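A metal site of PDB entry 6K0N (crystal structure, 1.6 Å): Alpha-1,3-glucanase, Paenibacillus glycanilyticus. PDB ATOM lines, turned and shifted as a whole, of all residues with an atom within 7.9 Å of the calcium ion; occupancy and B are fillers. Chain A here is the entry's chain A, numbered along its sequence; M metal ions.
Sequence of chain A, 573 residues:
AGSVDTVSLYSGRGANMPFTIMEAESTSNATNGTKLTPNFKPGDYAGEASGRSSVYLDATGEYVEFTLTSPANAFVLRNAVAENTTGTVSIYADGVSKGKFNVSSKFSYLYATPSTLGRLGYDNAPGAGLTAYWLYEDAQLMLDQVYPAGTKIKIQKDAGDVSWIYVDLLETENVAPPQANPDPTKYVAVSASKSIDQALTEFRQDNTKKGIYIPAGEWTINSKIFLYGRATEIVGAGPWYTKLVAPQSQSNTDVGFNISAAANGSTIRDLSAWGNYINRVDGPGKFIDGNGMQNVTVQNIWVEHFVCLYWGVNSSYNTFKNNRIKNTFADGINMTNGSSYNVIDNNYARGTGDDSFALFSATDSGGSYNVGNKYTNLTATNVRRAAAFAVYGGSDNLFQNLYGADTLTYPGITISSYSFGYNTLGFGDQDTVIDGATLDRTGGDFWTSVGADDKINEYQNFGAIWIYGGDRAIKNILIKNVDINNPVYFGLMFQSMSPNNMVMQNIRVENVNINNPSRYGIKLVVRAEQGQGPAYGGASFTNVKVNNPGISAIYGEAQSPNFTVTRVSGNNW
The backbone carbonyl oxygen of Asp 168 lies close to the backbone NH of Ala 24 (3.0 Å).
NH1 of Arg 78 is in salt-bridge range of OD2 of Asp 168 (2.8 Å).
The side-chain amide nitrogen of Asn 382 lies close to the backbone NH of Ser 50, at 3.3 Å.
Within 4 Å of the calcium ion: Glu 23, Glu 25, Ser 50, Ser 53 and Asp 168.
The nearest printed residue that does not touch the calcium ion is Ser 54 (4.4 Å).
OD1 of Asp 168 is bound to the calcium ion, 2.3 Å away.
The calcium ion is bound by OE1 of Glu 23, at 2.3 Å.
The calcium ion is bound by O of Ser 50 (2.3 Å).
O of Ser 53 binds the calcium ion, at 2.4 Å.
OE1 of Glu 25 binds the calcium ion (2.5 Å).
OE2 of Glu 25 is bound to the calcium ion, at 2.5 Å.
O of Asp 168 is bound to the calcium ion (2.6 Å).
The calcium ion has seven donor atoms within binding distance.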
ATOM      1  N   ILE A  21     -11.954 -15.167  -1.296  1.00  0.00           N
ATOM      2  CA  ILE A  21     -13.185 -15.240  -2.063  1.00  0.00           C
ATOM      3  C   ILE A  21     -13.327 -13.965  -2.879  1.00  0.00           C
ATOM      4  O   ILE A  21     -13.320 -12.865  -2.316  1.00  0.00           O
ATOM      5  CB  ILE A  21     -14.403 -15.423  -1.147  1.00  0.00           C
ATOM      6  CG1 ILE A  21     -14.249 -16.667  -0.263  1.00  0.00           C
ATOM      7  CG2 ILE A  21     -15.693 -15.412  -1.979  1.00  0.00           C
ATOM      8  CD1 ILE A  21     -14.830 -17.916  -0.839  1.00  0.00           C
ATOM      9  N   MET A  22     -13.474 -14.109  -4.199  1.00  0.00           N
ATOM     10  CA  MET A  22     -13.618 -12.952  -5.080  1.00  0.00           C
ATOM     11  C   MET A  22     -14.886 -13.091  -5.903  1.00  0.00           C
ATOM     12  O   MET A  22     -15.092 -14.109  -6.580  1.00  0.00           O
ATOM     13  CB  MET A  22     -12.385 -12.786  -5.966  1.00  0.00           C
ATOM     14  CG  MET A  22     -11.110 -12.586  -5.135  1.00  0.00           C
ATOM     15  SD  MET A  22      -9.773 -11.908  -6.127  1.00  0.00           S
ATOM     16  CE  MET A  22      -9.605 -13.193  -7.372  1.00  0.00           C
ATOM     17  N   GLU A  23     -15.755 -12.078  -5.842  1.00  0.00           N
ATOM     18  CA  GLU A  23     -17.000 -12.103  -6.600  1.00  0.00           C
ATOM     19  C   GLU A  23     -16.745 -11.809  -8.066  1.00  0.00           C
ATOM     20  O   GLU A  23     -16.037 -10.854  -8.400  1.00  0.00           O
ATOM     21  CB  GLU A  23     -17.992 -11.087  -6.037  1.00  0.00           C
ATOM     22  CG  GLU A  23     -18.410 -11.354  -4.587  1.00  0.00           C
ATOM     23  CD  GLU A  23     -19.315 -12.573  -4.425  1.00  0.00           C
ATOM     24  OE1 GLU A  23     -19.747 -13.170  -5.440  1.00  0.00           O
ATOM     25  OE2 GLU A  23     -19.597 -12.930  -3.254  1.00  0.00           O
ATOM     26  N   ALA A  24     -17.344 -12.616  -8.947  1.00  0.00           N
ATOM     27  CA  ALA A  24     -17.138 -12.402 -10.380  1.00  0.00           C
ATOM     28  C   ALA A  24     -17.597 -11.014 -10.811  1.00  0.00           C
ATOM     29  O   ALA A  24     -16.955 -10.369 -11.642  1.00  0.00           O
ATOM     30  CB  ALA A  24     -17.891 -13.476 -11.174  1.00  0.00           C
ATOM     31  N   GLU A  25     -18.706 -10.542 -10.241  1.00  0.00           N
ATOM     32  CA  GLU A  25     -19.376  -9.328 -10.673  1.00  0.00           C
ATOM     33  C   GLU A  25     -18.735  -8.061 -10.154  1.00  0.00           C
ATOM     34  O   GLU A  25     -19.252  -6.971 -10.421  1.00  0.00           O
ATOM     35  CB  GLU A  25     -20.846  -9.378 -10.238  1.00  0.00           C
ATOM     36  CG  GLU A  25     -21.037  -9.393  -8.725  1.00  0.00           C
ATOM     37  CD  GLU A  25     -21.066 -10.800  -8.109  1.00  0.00           C
ATOM     38  OE1 GLU A  25     -20.571 -11.763  -8.735  1.00  0.00           O
ATOM     39  OE2 GLU A  25     -21.605 -10.931  -6.989  1.00  0.00           O
ATOM     40  N   SER A  26     -17.631  -8.160  -9.404  1.00  0.00           N
ATOM     41  CA  SER A  26     -16.946  -6.980  -8.902  1.00  0.00           C
ATOM     42  C   SER A  26     -16.664  -5.986 -10.031  1.00  0.00           C
ATOM     43  O   SER A  26     -16.293  -6.377 -11.141  1.00  0.00           O
ATOM     44  CB  SER A  26     -15.644  -7.372  -8.225  1.00  0.00           C
ATOM     45  OG  SER A  26     -14.889  -6.218  -7.913  1.00  0.00           O
ATOM     46  N   TYR A  45     -30.952 -17.352 -10.961  1.00  0.00           N
ATOM     47  CA  TYR A  45     -29.487 -17.353 -11.033  1.00  0.00           C
ATOM     48  C   TYR A  45     -28.876 -16.139 -10.349  1.00  0.00           C
ATOM     49  O   TYR A  45     -27.718 -16.215  -9.941  1.00  0.00           O
ATOM     50  CB  TYR A  45     -29.014 -17.447 -12.489  1.00  0.00           C
ATOM     51  CG  TYR A  45     -29.336 -18.800 -13.085  1.00  0.00           C
ATOM     52  CD1 TYR A  45     -28.639 -19.947 -12.684  1.00  0.00           C
ATOM     53  CD2 TYR A  45     -30.347 -18.948 -14.028  1.00  0.00           C
ATOM     54  CE1 TYR A  45     -28.951 -21.186 -13.212  1.00  0.00           C
ATOM     55  CE2 TYR A  45     -30.652 -20.175 -14.555  1.00  0.00           C
ATOM     56  CZ  TYR A  45     -29.955 -21.297 -14.150  1.00  0.00           C
ATOM     57  OH  TYR A  45     -30.303 -22.516 -14.709  1.00  0.00           O
ATOM     58  N   ALA A  46     -29.611 -15.032 -10.218  1.00  0.00           N
ATOM     59  CA  ALA A  46     -29.089 -13.945  -9.387  1.00  0.00           C
ATOM     60  C   ALA A  46     -29.397 -14.178  -7.918  1.00  0.00           C
ATOM     61  O   ALA A  46     -28.509 -14.095  -7.062  1.00  0.00           O
ATOM     62  CB  ALA A  46     -29.673 -12.593  -9.834  1.00  0.00           C
ATOM     63  N   GLU A  48     -29.791 -16.696  -6.138  1.00  0.00           N
ATOM     64  CA  GLU A  48     -29.064 -17.772  -5.465  1.00  0.00           C
ATOM     65  C   GLU A  48     -27.552 -17.590  -5.518  1.00  0.00           C
ATOM     66  O   GLU A  48     -26.829 -18.424  -4.969  1.00  0.00           O
ATOM     67  CB  GLU A  48     -29.429 -19.123  -6.100  1.00  0.00           C
ATOM     68  CG  GLU A  48     -30.883 -19.532  -5.830  1.00  0.00           C
ATOM     69  CD  GLU A  48     -31.108 -21.020  -5.961  1.00  0.00           C
ATOM     70  OE1 GLU A  48     -30.119 -21.746  -6.199  1.00  0.00           O
ATOM     71  OE2 GLU A  48     -32.272 -21.464  -5.803  1.00  0.00           O
ATOM     72  N   ALA A  49     -27.064 -16.534  -6.144  1.00  0.00           N
ATOM     73  CA  ALA A  49     -25.623 -16.296  -6.216  1.00  0.00           C
ATOM     74  C   ALA A  49     -25.103 -15.612  -4.957  1.00  0.00           C
ATOM     75  O   ALA A  49     -25.818 -14.868  -4.283  1.00  0.00           O
ATOM     76  CB  ALA A  49     -25.298 -15.435  -7.445  1.00  0.00           C
ATOM     77  N   SER A  50     -23.834 -15.891  -4.643  1.00  0.00           N
ATOM     78  CA  SER A  50     -23.087 -15.021  -3.735  1.00  0.00           C
ATOM     79  C   SER A  50     -23.163 -13.562  -4.185  1.00  0.00           C
ATOM     80  O   SER A  50     -22.868 -13.254  -5.336  1.00  0.00           O
ATOM     81  CB  SER A  50     -21.629 -15.451  -3.703  1.00  0.00           C
ATOM     82  OG  SER A  50     -21.009 -14.950  -2.515  1.00  0.00           O
ATOM     83  N   GLY A  51     -23.483 -12.667  -3.236  1.00  0.00           N
ATOM     84  CA  GLY A  51     -23.644 -11.277  -3.613  1.00  0.00           C
ATOM     85  C   GLY A  51     -24.893 -10.991  -4.407  1.00  0.00           C
ATOM     86  O   GLY A  51     -25.089  -9.854  -4.863  1.00  0.00           O
ATOM     87  N   ARG A  52     -25.762 -11.991  -4.571  1.00  0.00           N
ATOM     88  CA  ARG A  52     -26.967 -11.914  -5.398  1.00  0.00           C
ATOM     89  C   ARG A  52     -26.654 -11.549  -6.848  1.00  0.00           C
ATOM     90  O   ARG A  52     -27.513 -11.013  -7.558  1.00  0.00           O
ATOM     91  CB  ARG A  52     -28.008 -10.954  -4.799  1.00  0.00           C
ATOM     92  CG  ARG A  52     -28.296 -11.223  -3.310  1.00  0.00           C
ATOM     93  CD  ARG A  52     -28.905 -12.617  -3.068  1.00  0.00           C
ATOM     94  NE  ARG A  52     -29.121 -12.810  -1.642  1.00  0.00           N
ATOM     95  CZ  ARG A  52     -30.112 -13.534  -1.096  1.00  0.00           C
ATOM     96  NH1 ARG A  52     -30.988 -14.185  -1.850  1.00  0.00           N
ATOM     97  NH2 ARG A  52     -30.215 -13.583   0.233  1.00  0.00           N
ATOM     98  N   SER A  53     -25.453 -11.874  -7.325  1.00  0.00           N
ATOM     99  CA  SER A  53     -25.154 -11.623  -8.724  1.00  0.00           C
ATOM    100  C   SER A  53     -24.062 -12.576  -9.208  1.00  0.00           C
ATOM    101  O   SER A  53     -23.267 -13.095  -8.417  1.00  0.00           O
ATOM    102  CB  SER A  53     -24.735 -10.165  -8.930  1.00  0.00           C
ATOM    103  OG  SER A  53     -24.325  -9.914 -10.273  1.00  0.00           O
ATOM    104  N   SER A  54     -24.053 -12.782 -10.515  1.00  0.00           N
ATOM    105  CA  SER A  54     -22.997 -13.530 -11.181  1.00  0.00           C
ATOM    106  C   SER A  54     -22.795 -12.919 -12.566  1.00  0.00           C
ATOM    107  O   SER A  54     -23.521 -12.023 -12.975  1.00  0.00           O
ATOM    108  CB  SER A  54     -23.328 -15.018 -11.266  1.00  0.00           C
ATOM    109  OG  SER A  54     -24.565 -15.196 -11.935  1.00  0.00           O
ATOM    110  N   VAL A  55     -21.785 -13.412 -13.274  1.00  0.00           N
ATOM    111  CA  VAL A  55     -21.546 -12.992 -14.653  1.00  0.00           C
ATOM    112  C   VAL A  55     -21.839 -14.179 -15.546  1.00  0.00           C
ATOM    113  O   VAL A  55     -21.256 -15.261 -15.386  1.00  0.00           O
ATOM    114  CB  VAL A  55     -20.115 -12.475 -14.872  1.00  0.00           C
ATOM    115  CG1 VAL A  55     -19.950 -12.027 -16.327  1.00  0.00           C
ATOM    116  CG2 VAL A  55     -19.844 -11.318 -13.913  1.00  0.00           C
ATOM    117  N   ARG A  78     -17.347 -21.243  -8.229  1.00  0.00           N
ATOM    118  CA  ARG A  78     -18.770 -21.466  -7.986  1.00  0.00           C
ATOM    119  C   ARG A  78     -19.529 -20.998  -9.226  1.00  0.00           C
ATOM    120  O   ARG A  78     -19.347 -19.853  -9.663  1.00  0.00           O
ATOM    121  CB  ARG A  78     -19.278 -20.737  -6.743  1.00  0.00           C
ATOM    122  CG  ARG A  78     -20.711 -21.171  -6.332  1.00  0.00           C
ATOM    123  CD  ARG A  78     -21.159 -20.500  -5.051  1.00  0.00           C
ATOM    124  NE  ARG A  78     -22.286 -21.201  -4.421  1.00  0.00           N
ATOM    125  CZ  ARG A  78     -23.537 -20.744  -4.354  1.00  0.00           C
ATOM    126  NH1 ARG A  78     -23.884 -19.583  -4.913  1.00  0.00           N
ATOM    127  NH2 ARG A  78     -24.463 -21.467  -3.733  1.00  0.00           N
ATOM    128  N   TYR A 136     -26.474 -23.514  -8.074  1.00  0.00           N
ATOM    129  CA  TYR A 136     -25.031 -23.365  -8.154  1.00  0.00           C
ATOM    130  C   TYR A 136     -24.303 -24.583  -7.610  1.00  0.00           C
ATOM    131  O   TYR A 136     -24.803 -25.285  -6.726  1.00  0.00           O
ATOM    132  CB  TYR A 136     -24.590 -22.093  -7.404  1.00  0.00           C
ATOM    133  CG  TYR A 136     -24.889 -20.852  -8.217  1.00  0.00           C
ATOM    134  CD1 TYR A 136     -23.974 -20.402  -9.163  1.00  0.00           C
ATOM    135  CD2 TYR A 136     -26.107 -20.188  -8.096  1.00  0.00           C
ATOM    136  CE1 TYR A 136     -24.227 -19.302  -9.952  1.00  0.00           C
ATOM    137  CE2 TYR A 136     -26.369 -19.059  -8.885  1.00  0.00           C
ATOM    138  CZ  TYR A 136     -25.429 -18.640  -9.817  1.00  0.00           C
ATOM    139  OH  TYR A 136     -25.674 -17.544 -10.603  1.00  0.00           O
ATOM    140  N   VAL A 167     -20.946 -17.502 -13.749  1.00  0.00           N
ATOM    141  CA  VAL A 167     -19.755 -17.482 -12.904  1.00  0.00           C
ATOM    142  C   VAL A 167     -20.059 -16.614 -11.693  1.00  0.00           C
ATOM    143  O   VAL A 167     -20.267 -15.401 -11.832  1.00  0.00           O
ATOM    144  CB  VAL A 167     -18.533 -16.958 -13.669  1.00  0.00           C
ATOM    145  CG1 VAL A 167     -17.327 -16.886 -12.736  1.00  0.00           C
ATOM    146  CG2 VAL A 167     -18.236 -17.839 -14.880  1.00  0.00           C
ATOM    147  N   ASP A 168     -20.093 -17.222 -10.515  1.00  0.00           N
ATOM    148  CA  ASP A 168     -20.543 -16.524  -9.307  1.00  0.00           C
ATOM    149  C   ASP A 168     -19.373 -15.932  -8.538  1.00  0.00           C
ATOM    150  O   ASP A 168     -19.364 -14.726  -8.234  1.00  0.00           O
ATOM    151  CB  ASP A 168     -21.328 -17.513  -8.426  1.00  0.00           C
ATOM    152  CG  ASP A 168     -21.888 -16.877  -7.163  1.00  0.00           C
ATOM    153  OD1 ASP A 168     -21.815 -15.643  -7.046  1.00  0.00           O
ATOM    154  OD2 ASP A 168     -22.405 -17.609  -6.305  1.00  0.00           O
ATOM    155  N   LEU A 169     -18.400 -16.760  -8.182  1.00  0.00           N
ATOM    156  CA  LEU A 169     -17.245 -16.321  -7.439  1.00  0.00           C
ATOM    157  C   LEU A 169     -16.099 -17.262  -7.724  1.00  0.00           C
ATOM    158  O   LEU A 169     -16.281 -18.363  -8.257  1.00  0.00           O
ATOM    159  CB  LEU A 169     -17.517 -16.283  -5.925  1.00  0.00           C
ATOM    160  CG  LEU A 169     -17.887 -17.617  -5.229  1.00  0.00           C
ATOM    161  CD1 LEU A 169     -16.691 -18.528  -4.894  1.00  0.00           C
ATOM    162  CD2 LEU A 169     -18.639 -17.304  -3.945  1.00  0.00           C
ATOM    163  N   LEU A 170     -14.904 -16.831  -7.330  1.00  0.00           N
ATOM    164  CA  LEU A 170     -13.685 -17.634  -7.436  1.00  0.00           C
ATOM    165  C   LEU A 170     -13.011 -17.662  -6.077  1.00  0.00           C
ATOM    166  O   LEU A 170     -12.756 -16.595  -5.504  1.00  0.00           O
ATOM    167  CB  LEU A 170     -12.753 -17.019  -8.486  1.00  0.00           C
ATOM    168  CG  LEU A 170     -11.453 -17.763  -8.755  1.00  0.00           C
ATOM    169  CD1 LEU A 170     -11.745 -19.045  -9.519  1.00  0.00           C
ATOM    170  CD2 LEU A 170     -10.518 -16.861  -9.554  1.00  0.00           C
ATOM    171  N   ASN A 382     -24.382 -18.350   1.512  1.00  0.00           N
ATOM    172  CA  ASN A 382     -25.160 -19.111   0.538  1.00  0.00           C
ATOM    173  C   ASN A 382     -25.913 -20.257   1.227  1.00  0.00           C
ATOM    174  O   ASN A 382     -25.791 -21.428   0.866  1.00  0.00           O
ATOM    175  CB  ASN A 382     -24.274 -19.650  -0.586  1.00  0.00           C
ATOM    176  CG  ASN A 382     -23.798 -18.577  -1.522  1.00  0.00           C
ATOM    177  OD1 ASN A 382     -22.594 -18.389  -1.709  1.00  0.00           O
ATOM    178  ND2 ASN A 382     -24.736 -17.862  -2.160  1.00  0.00           N
ATOM    179  N   ASP A 406     -26.358 -14.101   2.468  1.00  0.00           N
ATOM    180  CA  ASP A 406     -27.067 -14.676   1.329  1.00  0.00           C
ATOM    181  C   ASP A 406     -27.823 -15.953   1.690  1.00  0.00           C
ATOM    182  O   ASP A 406     -27.566 -17.047   1.182  1.00  0.00           O
ATOM    183  CB  ASP A 406     -26.084 -14.903   0.167  1.00  0.00           C
ATOM    184  CG  ASP A 406     -25.597 -13.598  -0.415  1.00  0.00           C
ATOM    185  OD1 ASP A 406     -26.446 -12.706  -0.609  1.00  0.00           O
ATOM    186  OD2 ASP A 406     -24.382 -13.438  -0.662  1.00  0.00           O
ATOM    187  N   ARG A 441     -27.329  -9.326   3.454  1.00  0.00           N
ATOM    188  CA  ARG A 441     -28.392  -9.853   2.614  1.00  0.00           C
ATOM    189  C   ARG A 441     -28.989 -11.138   3.192  1.00  0.00           C
ATOM    190  O   ARG A 441     -29.115 -12.167   2.515  1.00  0.00           O
ATOM    191  CB  ARG A 441     -27.884 -10.073   1.168  1.00  0.00           C
ATOM    192  CG  ARG A 441     -27.372  -8.778   0.490  1.00  0.00           C
ATOM    193  CD  ARG A 441     -26.654  -9.046  -0.851  1.00  0.00           C
ATOM    194  NE  ARG A 441     -25.588 -10.017  -0.666  1.00  0.00           N
ATOM    195  CZ  ARG A 441     -24.359  -9.736  -0.236  1.00  0.00           C
ATOM    196  NH1 ARG A 441     -24.017  -8.471   0.010  1.00  0.00           N
ATOM    197  NH2 ARG A 441     -23.473 -10.704  -0.055  1.00  0.00           N
HETATM  198 CA    CA M   1     -21.320 -13.432  -7.095  1.00  0.00          CA
